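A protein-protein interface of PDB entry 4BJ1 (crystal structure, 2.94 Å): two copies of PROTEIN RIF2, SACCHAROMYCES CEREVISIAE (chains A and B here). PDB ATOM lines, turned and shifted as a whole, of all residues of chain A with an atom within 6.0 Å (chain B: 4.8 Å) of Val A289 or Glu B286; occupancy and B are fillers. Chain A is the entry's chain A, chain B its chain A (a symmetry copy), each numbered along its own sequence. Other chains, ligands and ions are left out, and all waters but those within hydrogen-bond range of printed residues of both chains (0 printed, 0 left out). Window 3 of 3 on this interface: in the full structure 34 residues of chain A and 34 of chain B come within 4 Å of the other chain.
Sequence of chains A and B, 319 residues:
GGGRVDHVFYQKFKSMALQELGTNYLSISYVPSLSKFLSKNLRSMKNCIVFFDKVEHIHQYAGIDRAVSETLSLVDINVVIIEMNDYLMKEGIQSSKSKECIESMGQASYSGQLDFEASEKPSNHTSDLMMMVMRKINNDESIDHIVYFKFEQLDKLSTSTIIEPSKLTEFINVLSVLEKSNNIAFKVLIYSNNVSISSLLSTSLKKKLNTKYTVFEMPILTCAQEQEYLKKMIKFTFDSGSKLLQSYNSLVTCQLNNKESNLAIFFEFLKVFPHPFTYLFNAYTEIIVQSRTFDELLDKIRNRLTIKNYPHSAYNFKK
The backbone carbonyl oxygen of Val A289 sits at hydrogen-bond distance from the side-chain amino group of Lys A14 (3.1 Å). The side-chain hydroxyl (OG1) of Thr B285 lies within hydrogen-bond range of the backbone carbonyl oxygen (O) of Asn B282 (3.2 Å). OE1 of Glu B286 sits at hydrogen-bond distance from NE2 of His B312, at 3.0 Å.
NZ of Lys A14 touches OD1 of Asn B282 (3.7 Å). Val B289 touches Thr A285 (CG2 to OG1, 3.8 Å). Glu A286 touches Val B289 (CG to CG1, 3.8 Å). Thr B285 touches Val A289. Val A289 touches Glu B286 (CG1 to CG, 3.8 Å). CG2 of Val A289 touches CG2 of Val B289 (3.99 Å).
Of the printed residues of chain B, Val A289 touches Thr B285 (3.8 Å), Glu B286 (3.8 Å) and Val B289 (3.99 Å). Ser A291 touches none of the printed residues of chain B. Of the printed residues of chain A, Asn B282 touches Lys A14 (3.7 Å). Tyr B284 touches none of the printed residues of chain A. Of the printed residues of chain A, Thr B285 touches Val A289 (3.8 Å). Glu B286 touches just one residue of chain A: Val A289 (3.8 Å). Printed residues of chain A within 4 Å of Val B289: Thr A285, Glu A286 and Val A289. The nearest residue of chain A that does not touch Glu B286 is Lys A14 (5.9 Å).
Of the 12 printed residues of chain A, 4 touch a printed residue of chain B. Of the 13 printed residues of chain B, 4 touch a printed residue of chain A. Hydrophobic or aromatic side chains of chain B within 4 Å of the printed part of chain A: Val B289. Among the printed residues, 6 pairs touch across the chains. Among the printed residues, no Asp or Glu carboxylate lies within 4 Å of a Lys or Arg side-chain nitrogen of the other chain.
Thr A285 touches Val B289, and with the chains exchanged Val A289 touches Thr B285. Glu A286 touches Val B289, and with the chains exchanged Val A289 touches Glu B286. Val A289 touches its own counterpart, Val B289. 8 positions are printed for both chains. Of the 6 pairs that touch across the chains among the printed residues, 5 have their exchanged pair printed and touching as well.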
ATOM      1  N   TYR A  10      -3.837   9.371  22.838  1.00  0.00           N
ATOM      2  CA  TYR A  10      -5.046   9.997  22.344  1.00  0.00           C
ATOM      3  C   TYR A  10      -4.684  10.973  21.224  1.00  0.00           C
ATOM      4  O   TYR A  10      -5.419  11.052  20.249  1.00  0.00           O
ATOM      5  CB  TYR A  10      -5.831  10.663  23.489  1.00  0.00           C
ATOM      6  CG  TYR A  10      -7.081  11.353  23.018  1.00  0.00           C
ATOM      7  CD1 TYR A  10      -8.108  10.636  22.407  1.00  0.00           C
ATOM      8  CD2 TYR A  10      -7.200  12.737  23.082  1.00  0.00           C
ATOM      9  CE1 TYR A  10      -9.220  11.283  21.869  1.00  0.00           C
ATOM     10  CE2 TYR A  10      -8.307  13.398  22.536  1.00  0.00           C
ATOM     11  CZ  TYR A  10      -9.310  12.666  21.929  1.00  0.00           C
ATOM     12  OH  TYR A  10     -10.411  13.318  21.437  1.00  0.00           O
ATOM     13  N   LYS A  14      -6.821  11.511  18.050  1.00  0.00           N
ATOM     14  CA  LYS A  14      -7.271  12.883  17.850  1.00  0.00           C
ATOM     15  C   LYS A  14      -6.889  13.367  16.467  1.00  0.00           C
ATOM     16  O   LYS A  14      -7.779  13.748  15.704  1.00  0.00           O
ATOM     17  CB  LYS A  14      -6.669  13.793  18.933  1.00  0.00           C
ATOM     18  CG  LYS A  14      -7.111  15.254  18.872  1.00  0.00           C
ATOM     19  CD  LYS A  14      -6.910  15.887  20.220  1.00  0.00           C
ATOM     20  CE  LYS A  14      -6.895  17.376  20.176  1.00  0.00           C
ATOM     21  NZ  LYS A  14      -6.434  17.897  21.480  1.00  0.00           N
ATOM     22  N   LEU A  18      -9.434  13.801  13.375  1.00  0.00           N
ATOM     23  CA  LEU A  18      -9.594  15.114  12.777  1.00  0.00           C
ATOM     24  C   LEU A  18      -9.396  15.099  11.276  1.00  0.00           C
ATOM     25  O   LEU A  18     -10.272  15.593  10.558  1.00  0.00           O
ATOM     26  CB  LEU A  18      -8.726  16.146  13.461  1.00  0.00           C
ATOM     27  CG  LEU A  18      -9.433  16.756  14.651  1.00  0.00           C
ATOM     28  CD1 LEU A  18      -8.487  17.005  15.792  1.00  0.00           C
ATOM     29  CD2 LEU A  18     -10.204  18.015  14.248  1.00  0.00           C
ATOM     30  N   TYR A 284     -18.808  18.187  16.062  1.00  0.00           N
ATOM     31  CA  TYR A 284     -17.904  17.062  16.220  1.00  0.00           C
ATOM     32  C   TYR A 284     -16.429  17.427  16.264  1.00  0.00           C
ATOM     33  O   TYR A 284     -15.711  16.837  17.076  1.00  0.00           O
ATOM     34  CB  TYR A 284     -18.171  16.012  15.160  1.00  0.00           C
ATOM     35  CG  TYR A 284     -18.373  14.650  15.764  1.00  0.00           C
ATOM     36  CD1 TYR A 284     -19.531  14.349  16.475  1.00  0.00           C
ATOM     37  CD2 TYR A 284     -17.393  13.663  15.650  1.00  0.00           C
ATOM     38  CE1 TYR A 284     -19.714  13.100  17.053  1.00  0.00           C
ATOM     39  CE2 TYR A 284     -17.562  12.412  16.229  1.00  0.00           C
ATOM     40  CZ  TYR A 284     -18.727  12.135  16.928  1.00  0.00           C
ATOM     41  OH  TYR A 284     -18.920  10.904  17.497  1.00  0.00           O
ATOM     42  N   THR A 285     -15.954  18.366  15.418  1.00  0.00           N
ATOM     43  CA  THR A 285     -14.544  18.769  15.494  1.00  0.00           C
ATOM     44  C   THR A 285     -14.259  19.364  16.898  1.00  0.00           C
ATOM     45  O   THR A 285     -13.234  19.047  17.485  1.00  0.00           O
ATOM     46  CB  THR A 285     -14.121  19.698  14.355  1.00  0.00           C
ATOM     47  OG1 THR A 285     -14.852  20.886  14.478  1.00  0.00           O
ATOM     48  CG2 THR A 285     -14.339  19.095  12.973  1.00  0.00           C
ATOM     49  N   GLU A 286     -15.221  20.115  17.467  1.00  0.00           N
ATOM     50  CA  GLU A 286     -15.120  20.670  18.819  1.00  0.00           C
ATOM     51  C   GLU A 286     -14.953  19.604  19.882  1.00  0.00           C
ATOM     52  O   GLU A 286     -13.994  19.689  20.638  1.00  0.00           O
ATOM     53  CB  GLU A 286     -16.319  21.555  19.151  1.00  0.00           C
ATOM     54  CG  GLU A 286     -16.219  22.936  18.542  1.00  0.00           C
ATOM     55  CD  GLU A 286     -17.402  23.830  18.838  1.00  0.00           C
ATOM     56  OE1 GLU A 286     -18.004  23.688  19.928  1.00  0.00           O
ATOM     57  OE2 GLU A 286     -17.713  24.694  17.986  1.00  0.00           O
ATOM     58  N   ILE A 287     -15.842  18.583  19.928  1.00  0.00           N
ATOM     59  CA  ILE A 287     -15.717  17.515  20.926  1.00  0.00           C
ATOM     60  C   ILE A 287     -14.356  16.827  20.808  1.00  0.00           C
ATOM     61  O   ILE A 287     -13.722  16.622  21.841  1.00  0.00           O
ATOM     62  CB  ILE A 287     -16.889  16.495  21.009  1.00  0.00           C
ATOM     63  CG1 ILE A 287     -17.032  15.660  19.727  1.00  0.00           C
ATOM     64  CG2 ILE A 287     -18.217  17.170  21.402  1.00  0.00           C
ATOM     65  CD1 ILE A 287     -17.904  14.490  19.837  1.00  0.00           C
ATOM     66  N   ILE A 288     -13.872  16.544  19.569  1.00  0.00           N
ATOM     67  CA  ILE A 288     -12.559  15.904  19.356  1.00  0.00           C
ATOM     68  C   ILE A 288     -11.444  16.812  19.850  1.00  0.00           C
ATOM     69  O   ILE A 288     -10.685  16.393  20.704  1.00  0.00           O
ATOM     70  CB  ILE A 288     -12.329  15.383  17.888  1.00  0.00           C
ATOM     71  CG1 ILE A 288     -13.429  14.337  17.501  1.00  0.00           C
ATOM     72  CG2 ILE A 288     -10.920  14.796  17.725  1.00  0.00           C
ATOM     73  CD1 ILE A 288     -13.634  14.088  16.095  1.00  0.00           C
ATOM     74  N   VAL A 289     -11.367  18.053  19.335  1.00  0.00           N
ATOM     75  CA  VAL A 289     -10.366  19.074  19.688  1.00  0.00           C
ATOM     76  C   VAL A 289     -10.329  19.336  21.218  1.00  0.00           C
ATOM     77  O   VAL A 289      -9.264  19.189  21.816  1.00  0.00           O
ATOM     78  CB  VAL A 289     -10.557  20.365  18.846  1.00  0.00           C
ATOM     79  CG1 VAL A 289      -9.938  21.579  19.513  1.00  0.00           C
ATOM     80  CG2 VAL A 289      -9.999  20.186  17.442  1.00  0.00           C
ATOM     81  N   GLN A 290     -11.488  19.669  21.842  1.00  0.00           N
ATOM     82  CA  GLN A 290     -11.594  19.971  23.275  1.00  0.00           C
ATOM     83  C   GLN A 290     -11.258  18.823  24.213  1.00  0.00           C
ATOM     84  O   GLN A 290     -10.918  19.092  25.356  1.00  0.00           O
ATOM     85  CB  GLN A 290     -12.977  20.479  23.626  1.00  0.00           C
ATOM     86  CG  GLN A 290     -13.352  21.802  22.991  1.00  0.00           C
ATOM     87  CD  GLN A 290     -14.853  21.989  22.966  1.00  0.00           C
ATOM     88  OE1 GLN A 290     -15.355  22.891  22.289  1.00  0.00           O
ATOM     89  NE2 GLN A 290     -15.612  21.141  23.689  1.00  0.00           N
ATOM     90  N   SER A 291     -11.406  17.566  23.777  1.00  0.00           N
ATOM     91  CA  SER A 291     -11.102  16.416  24.620  1.00  0.00           C
ATOM     92  C   SER A 291      -9.603  16.214  24.708  1.00  0.00           C
ATOM     93  O   SER A 291      -8.920  16.296  23.688  1.00  0.00           O
ATOM     94  CB  SER A 291     -11.766  15.149  24.095  1.00  0.00           C
ATOM     95  OG  SER A 291     -13.174  15.271  24.147  1.00  0.00           O
ATOM     96  N   ARG A 292      -9.093  15.948  25.927  1.00  0.00           N
ATOM     97  CA  ARG A 292      -7.669  15.738  26.157  1.00  0.00           C
ATOM     98  C   ARG A 292      -7.317  14.262  26.371  1.00  0.00           C
ATOM     99  O   ARG A 292      -6.141  13.891  26.322  1.00  0.00           O
ATOM    100  CB  ARG A 292      -7.178  16.635  27.290  1.00  0.00           C
ATOM    101  CG  ARG A 292      -7.110  18.103  26.861  1.00  0.00           C
ATOM    102  CD  ARG A 292      -6.331  18.962  27.838  1.00  0.00           C
ATOM    103  NE  ARG A 292      -4.919  18.578  27.909  1.00  0.00           N
ATOM    104  CZ  ARG A 292      -4.083  18.974  28.863  1.00  0.00           C
ATOM    105  NH1 ARG A 292      -4.505  19.774  29.836  1.00  0.00           N
ATOM    106  NH2 ARG A 292      -2.818  18.569  28.856  1.00  0.00           N
ATOM    107  N   ASN B 282      -2.039  21.144  18.242  1.00  0.00           N
ATOM    108  CA  ASN B 282      -3.149  21.418  19.140  1.00  0.00           C
ATOM    109  C   ASN B 282      -3.552  22.900  19.139  1.00  0.00           C
ATOM    110  O   ASN B 282      -4.747  23.226  19.011  1.00  0.00           O
ATOM    111  CB  ASN B 282      -2.869  20.885  20.540  1.00  0.00           C
ATOM    112  CG  ASN B 282      -2.719  19.378  20.603  1.00  0.00           C
ATOM    113  OD1 ASN B 282      -3.264  18.629  19.789  1.00  0.00           O
ATOM    114  ND2 ASN B 282      -1.968  18.889  21.580  1.00  0.00           N
ATOM    115  N   ALA B 283      -2.545  23.788  19.219  1.00  0.00           N
ATOM    116  CA  ALA B 283      -2.754  25.232  19.235  1.00  0.00           C
ATOM    117  C   ALA B 283      -3.450  25.675  17.949  1.00  0.00           C
ATOM    118  O   ALA B 283      -4.443  26.405  18.007  1.00  0.00           O
ATOM    119  CB  ALA B 283      -1.422  25.952  19.403  1.00  0.00           C
ATOM    120  N   TYR B 284      -2.974  25.161  16.799  1.00  0.00           N
ATOM    121  CA  TYR B 284      -3.487  25.519  15.489  1.00  0.00           C
ATOM    122  C   TYR B 284      -4.868  24.971  15.169  1.00  0.00           C
ATOM    123  O   TYR B 284      -5.662  25.711  14.582  1.00  0.00           O
ATOM    124  CB  TYR B 284      -2.492  25.144  14.408  1.00  0.00           C
ATOM    125  CG  TYR B 284      -2.188  26.306  13.504  1.00  0.00           C
ATOM    126  CD1 TYR B 284      -1.424  27.379  13.952  1.00  0.00           C
ATOM    127  CD2 TYR B 284      -2.687  26.349  12.201  1.00  0.00           C
ATOM    128  CE1 TYR B 284      -1.158  28.464  13.128  1.00  0.00           C
ATOM    129  CE2 TYR B 284      -2.432  27.433  11.370  1.00  0.00           C
ATOM    130  CZ  TYR B 284      -1.664  28.488  11.839  1.00  0.00           C
ATOM    131  OH  TYR B 284      -1.390  29.560  11.033  1.00  0.00           O
ATOM    132  N   THR B 285      -5.176  23.705  15.525  1.00  0.00           N
ATOM    133  CA  THR B 285      -6.528  23.187  15.276  1.00  0.00           C
ATOM    134  C   THR B 285      -7.555  24.047  16.057  1.00  0.00           C
ATOM    135  O   THR B 285      -8.593  24.388  15.506  1.00  0.00           O
ATOM    136  CB  THR B 285      -6.661  21.691  15.562  1.00  0.00           C
ATOM    137  OG1 THR B 285      -6.437  21.496  16.931  1.00  0.00           O
ATOM    138  CG2 THR B 285      -5.697  20.834  14.752  1.00  0.00           C
ATOM    139  N   GLU B 286      -7.202  24.489  17.280  1.00  0.00           N
ATOM    140  CA  GLU B 286      -8.038  25.375  18.093  1.00  0.00           C
ATOM    141  C   GLU B 286      -8.334  26.694  17.410  1.00  0.00           C
ATOM    142  O   GLU B 286      -9.506  27.025  17.279  1.00  0.00           O
ATOM    143  CB  GLU B 286      -7.419  25.625  19.465  1.00  0.00           C
ATOM    144  CG  GLU B 286      -7.639  24.481  20.429  1.00  0.00           C
ATOM    145  CD  GLU B 286      -7.019  24.691  21.793  1.00  0.00           C
ATOM    146  OE1 GLU B 286      -6.941  25.858  22.242  1.00  0.00           O
ATOM    147  OE2 GLU B 286      -6.634  23.681  22.425  1.00  0.00           O
ATOM    148  N   ILE B 287      -7.301  27.432  16.938  1.00  0.00           N
ATOM    149  CA  ILE B 287      -7.533  28.709  16.254  1.00  0.00           C
ATOM    150  C   ILE B 287      -8.441  28.510  15.040  1.00  0.00           C
ATOM    151  O   ILE B 287      -9.372  29.297  14.881  1.00  0.00           O
ATOM    152  CB  ILE B 287      -6.274  29.560  15.918  1.00  0.00           C
ATOM    153  CG1 ILE B 287      -5.351  28.867  14.903  1.00  0.00           C
ATOM    154  CG2 ILE B 287      -5.510  29.990  17.184  1.00  0.00           C
ATOM    155  CD1 ILE B 287      -4.317  29.718  14.314  1.00  0.00           C
ATOM    156  N   ILE B 288      -8.230  27.433  14.237  1.00  0.00           N
ATOM    157  CA  ILE B 288      -9.071  27.147  13.057  1.00  0.00           C
ATOM    158  C   ILE B 288     -10.499  26.853  13.486  1.00  0.00           C
ATOM    159  O   ILE B 288     -11.396  27.543  13.040  1.00  0.00           O
ATOM    160  CB  ILE B 288      -8.475  26.050  12.096  1.00  0.00           C
ATOM    161  CG1 ILE B 288      -7.066  26.490  11.572  1.00  0.00           C
ATOM    162  CG2 ILE B 288      -9.435  25.754  10.933  1.00  0.00           C
ATOM    163  CD1 ILE B 288      -6.207  25.455  11.050  1.00  0.00           C
ATOM    164  N   VAL B 289     -10.701  25.855  14.367  1.00  0.00           N
ATOM    165  CA  VAL B 289     -12.003  25.426  14.903  1.00  0.00           C
ATOM    166  C   VAL B 289     -12.778  26.609  15.543  1.00  0.00           C
ATOM    167  O   VAL B 289     -13.904  26.874  15.123  1.00  0.00           O
ATOM    168  CB  VAL B 289     -11.848  24.205  15.851  1.00  0.00           C
ATOM    169  CG1 VAL B 289     -13.019  24.072  16.806  1.00  0.00           C
ATOM    170  CG2 VAL B 289     -11.661  22.921  15.057  1.00  0.00           C
ATOM    171  N   GLN B 290     -12.160  27.335  16.510  1.00  0.00           N
ATOM    172  CA  GLN B 290     -12.782  28.459  17.219  1.00  0.00           C
ATOM    173  C   GLN B 290     -13.143  29.659  16.359  1.00  0.00           C
ATOM    174  O   GLN B 290     -14.010  30.420  16.764  1.00  0.00           O
ATOM    175  CB  GLN B 290     -11.905  28.942  18.357  1.00  0.00           C
ATOM    176  CG  GLN B 290     -11.692  27.938  19.470  1.00  0.00           C
ATOM    177  CD  GLN B 290     -10.456  28.271  20.277  1.00  0.00           C
ATOM    178  OE1 GLN B 290      -9.995  27.449  21.075  1.00  0.00           O
ATOM    179  NE2 GLN B 290      -9.879  29.475  20.089  1.00  0.00           N
ATOM    180  N   SER B 291     -12.463  29.871  15.226  1.00  0.00           N
ATOM    181  CA  SER B 291     -12.756  30.999  14.349  1.00  0.00           C
ATOM    182  C   SER B 291     -14.012  30.726  13.548  1.00  0.00           C
ATOM    183  O   SER B 291     -14.173  29.622  13.032  1.00  0.00           O
ATOM    184  CB  SER B 291     -11.593  31.290  13.408  1.00  0.00           C
ATOM    185  OG  SER B 291     -10.451  31.690  14.140  1.00  0.00           O
ATOM    186  N   TYR B 310      -2.700  29.391  23.863  1.00  0.00           N
ATOM    187  CA  TYR B 310      -2.963  28.175  23.096  1.00  0.00           C
ATOM    188  C   TYR B 310      -1.932  27.066  23.240  1.00  0.00           C
ATOM    189  O   TYR B 310      -0.735  27.342  23.170  1.00  0.00           O
ATOM    190  CB  TYR B 310      -3.058  28.533  21.604  1.00  0.00           C
ATOM    191  CG  TYR B 310      -4.307  29.293  21.233  1.00  0.00           C
ATOM    192  CD1 TYR B 310      -5.494  28.625  20.952  1.00  0.00           C
ATOM    193  CD2 TYR B 310      -4.301  30.681  21.144  1.00  0.00           C
ATOM    194  CE1 TYR B 310      -6.651  29.319  20.616  1.00  0.00           C
ATOM    195  CE2 TYR B 310      -5.454  31.389  20.796  1.00  0.00           C
ATOM    196  CZ  TYR B 310      -6.628  30.701  20.533  1.00  0.00           C
ATOM    197  OH  TYR B 310      -7.765  31.376  20.173  1.00  0.00           O
ATOM    198  N   PRO B 311      -2.346  25.782  23.305  1.00  0.00           N
ATOM    199  CA  PRO B 311      -3.716  25.243  23.408  1.00  0.00           C
ATOM    200  C   PRO B 311      -4.352  25.524  24.791  1.00  0.00           C
ATOM    201  O   PRO B 311      -3.710  26.138  25.637  1.00  0.00           O
ATOM    202  CB  PRO B 311      -3.497  23.728  23.186  1.00  0.00           C
ATOM    203  CG  PRO B 311      -2.059  23.553  22.766  1.00  0.00           C
ATOM    204  CD  PRO B 311      -1.354  24.694  23.378  1.00  0.00           C
ATOM    205  N   HIS B 312      -5.609  25.104  25.026  1.00  0.00           N
ATOM    206  CA  HIS B 312      -6.255  25.220  26.338  1.00  0.00           C
ATOM    207  C   HIS B 312      -7.094  23.994  26.633  1.00  0.00           C
ATOM    208  O   HIS B 312      -6.602  22.879  26.456  1.00  0.00           O
ATOM    209  CB  HIS B 312      -7.028  26.532  26.555  1.00  0.00           C
ATOM    210  CG  HIS B 312      -7.679  27.101  25.336  1.00  0.00           C
ATOM    211  ND1 HIS B 312      -7.201  28.258  24.740  1.00  0.00           N
ATOM    212  CD2 HIS B 312      -8.771  26.681  24.660  1.00  0.00           C
ATOM    213  CE1 HIS B 312      -8.005  28.494  23.715  1.00  0.00           C
ATOM    214  NE2 HIS B 312      -8.956  27.567  23.621  1.00  0.00           N
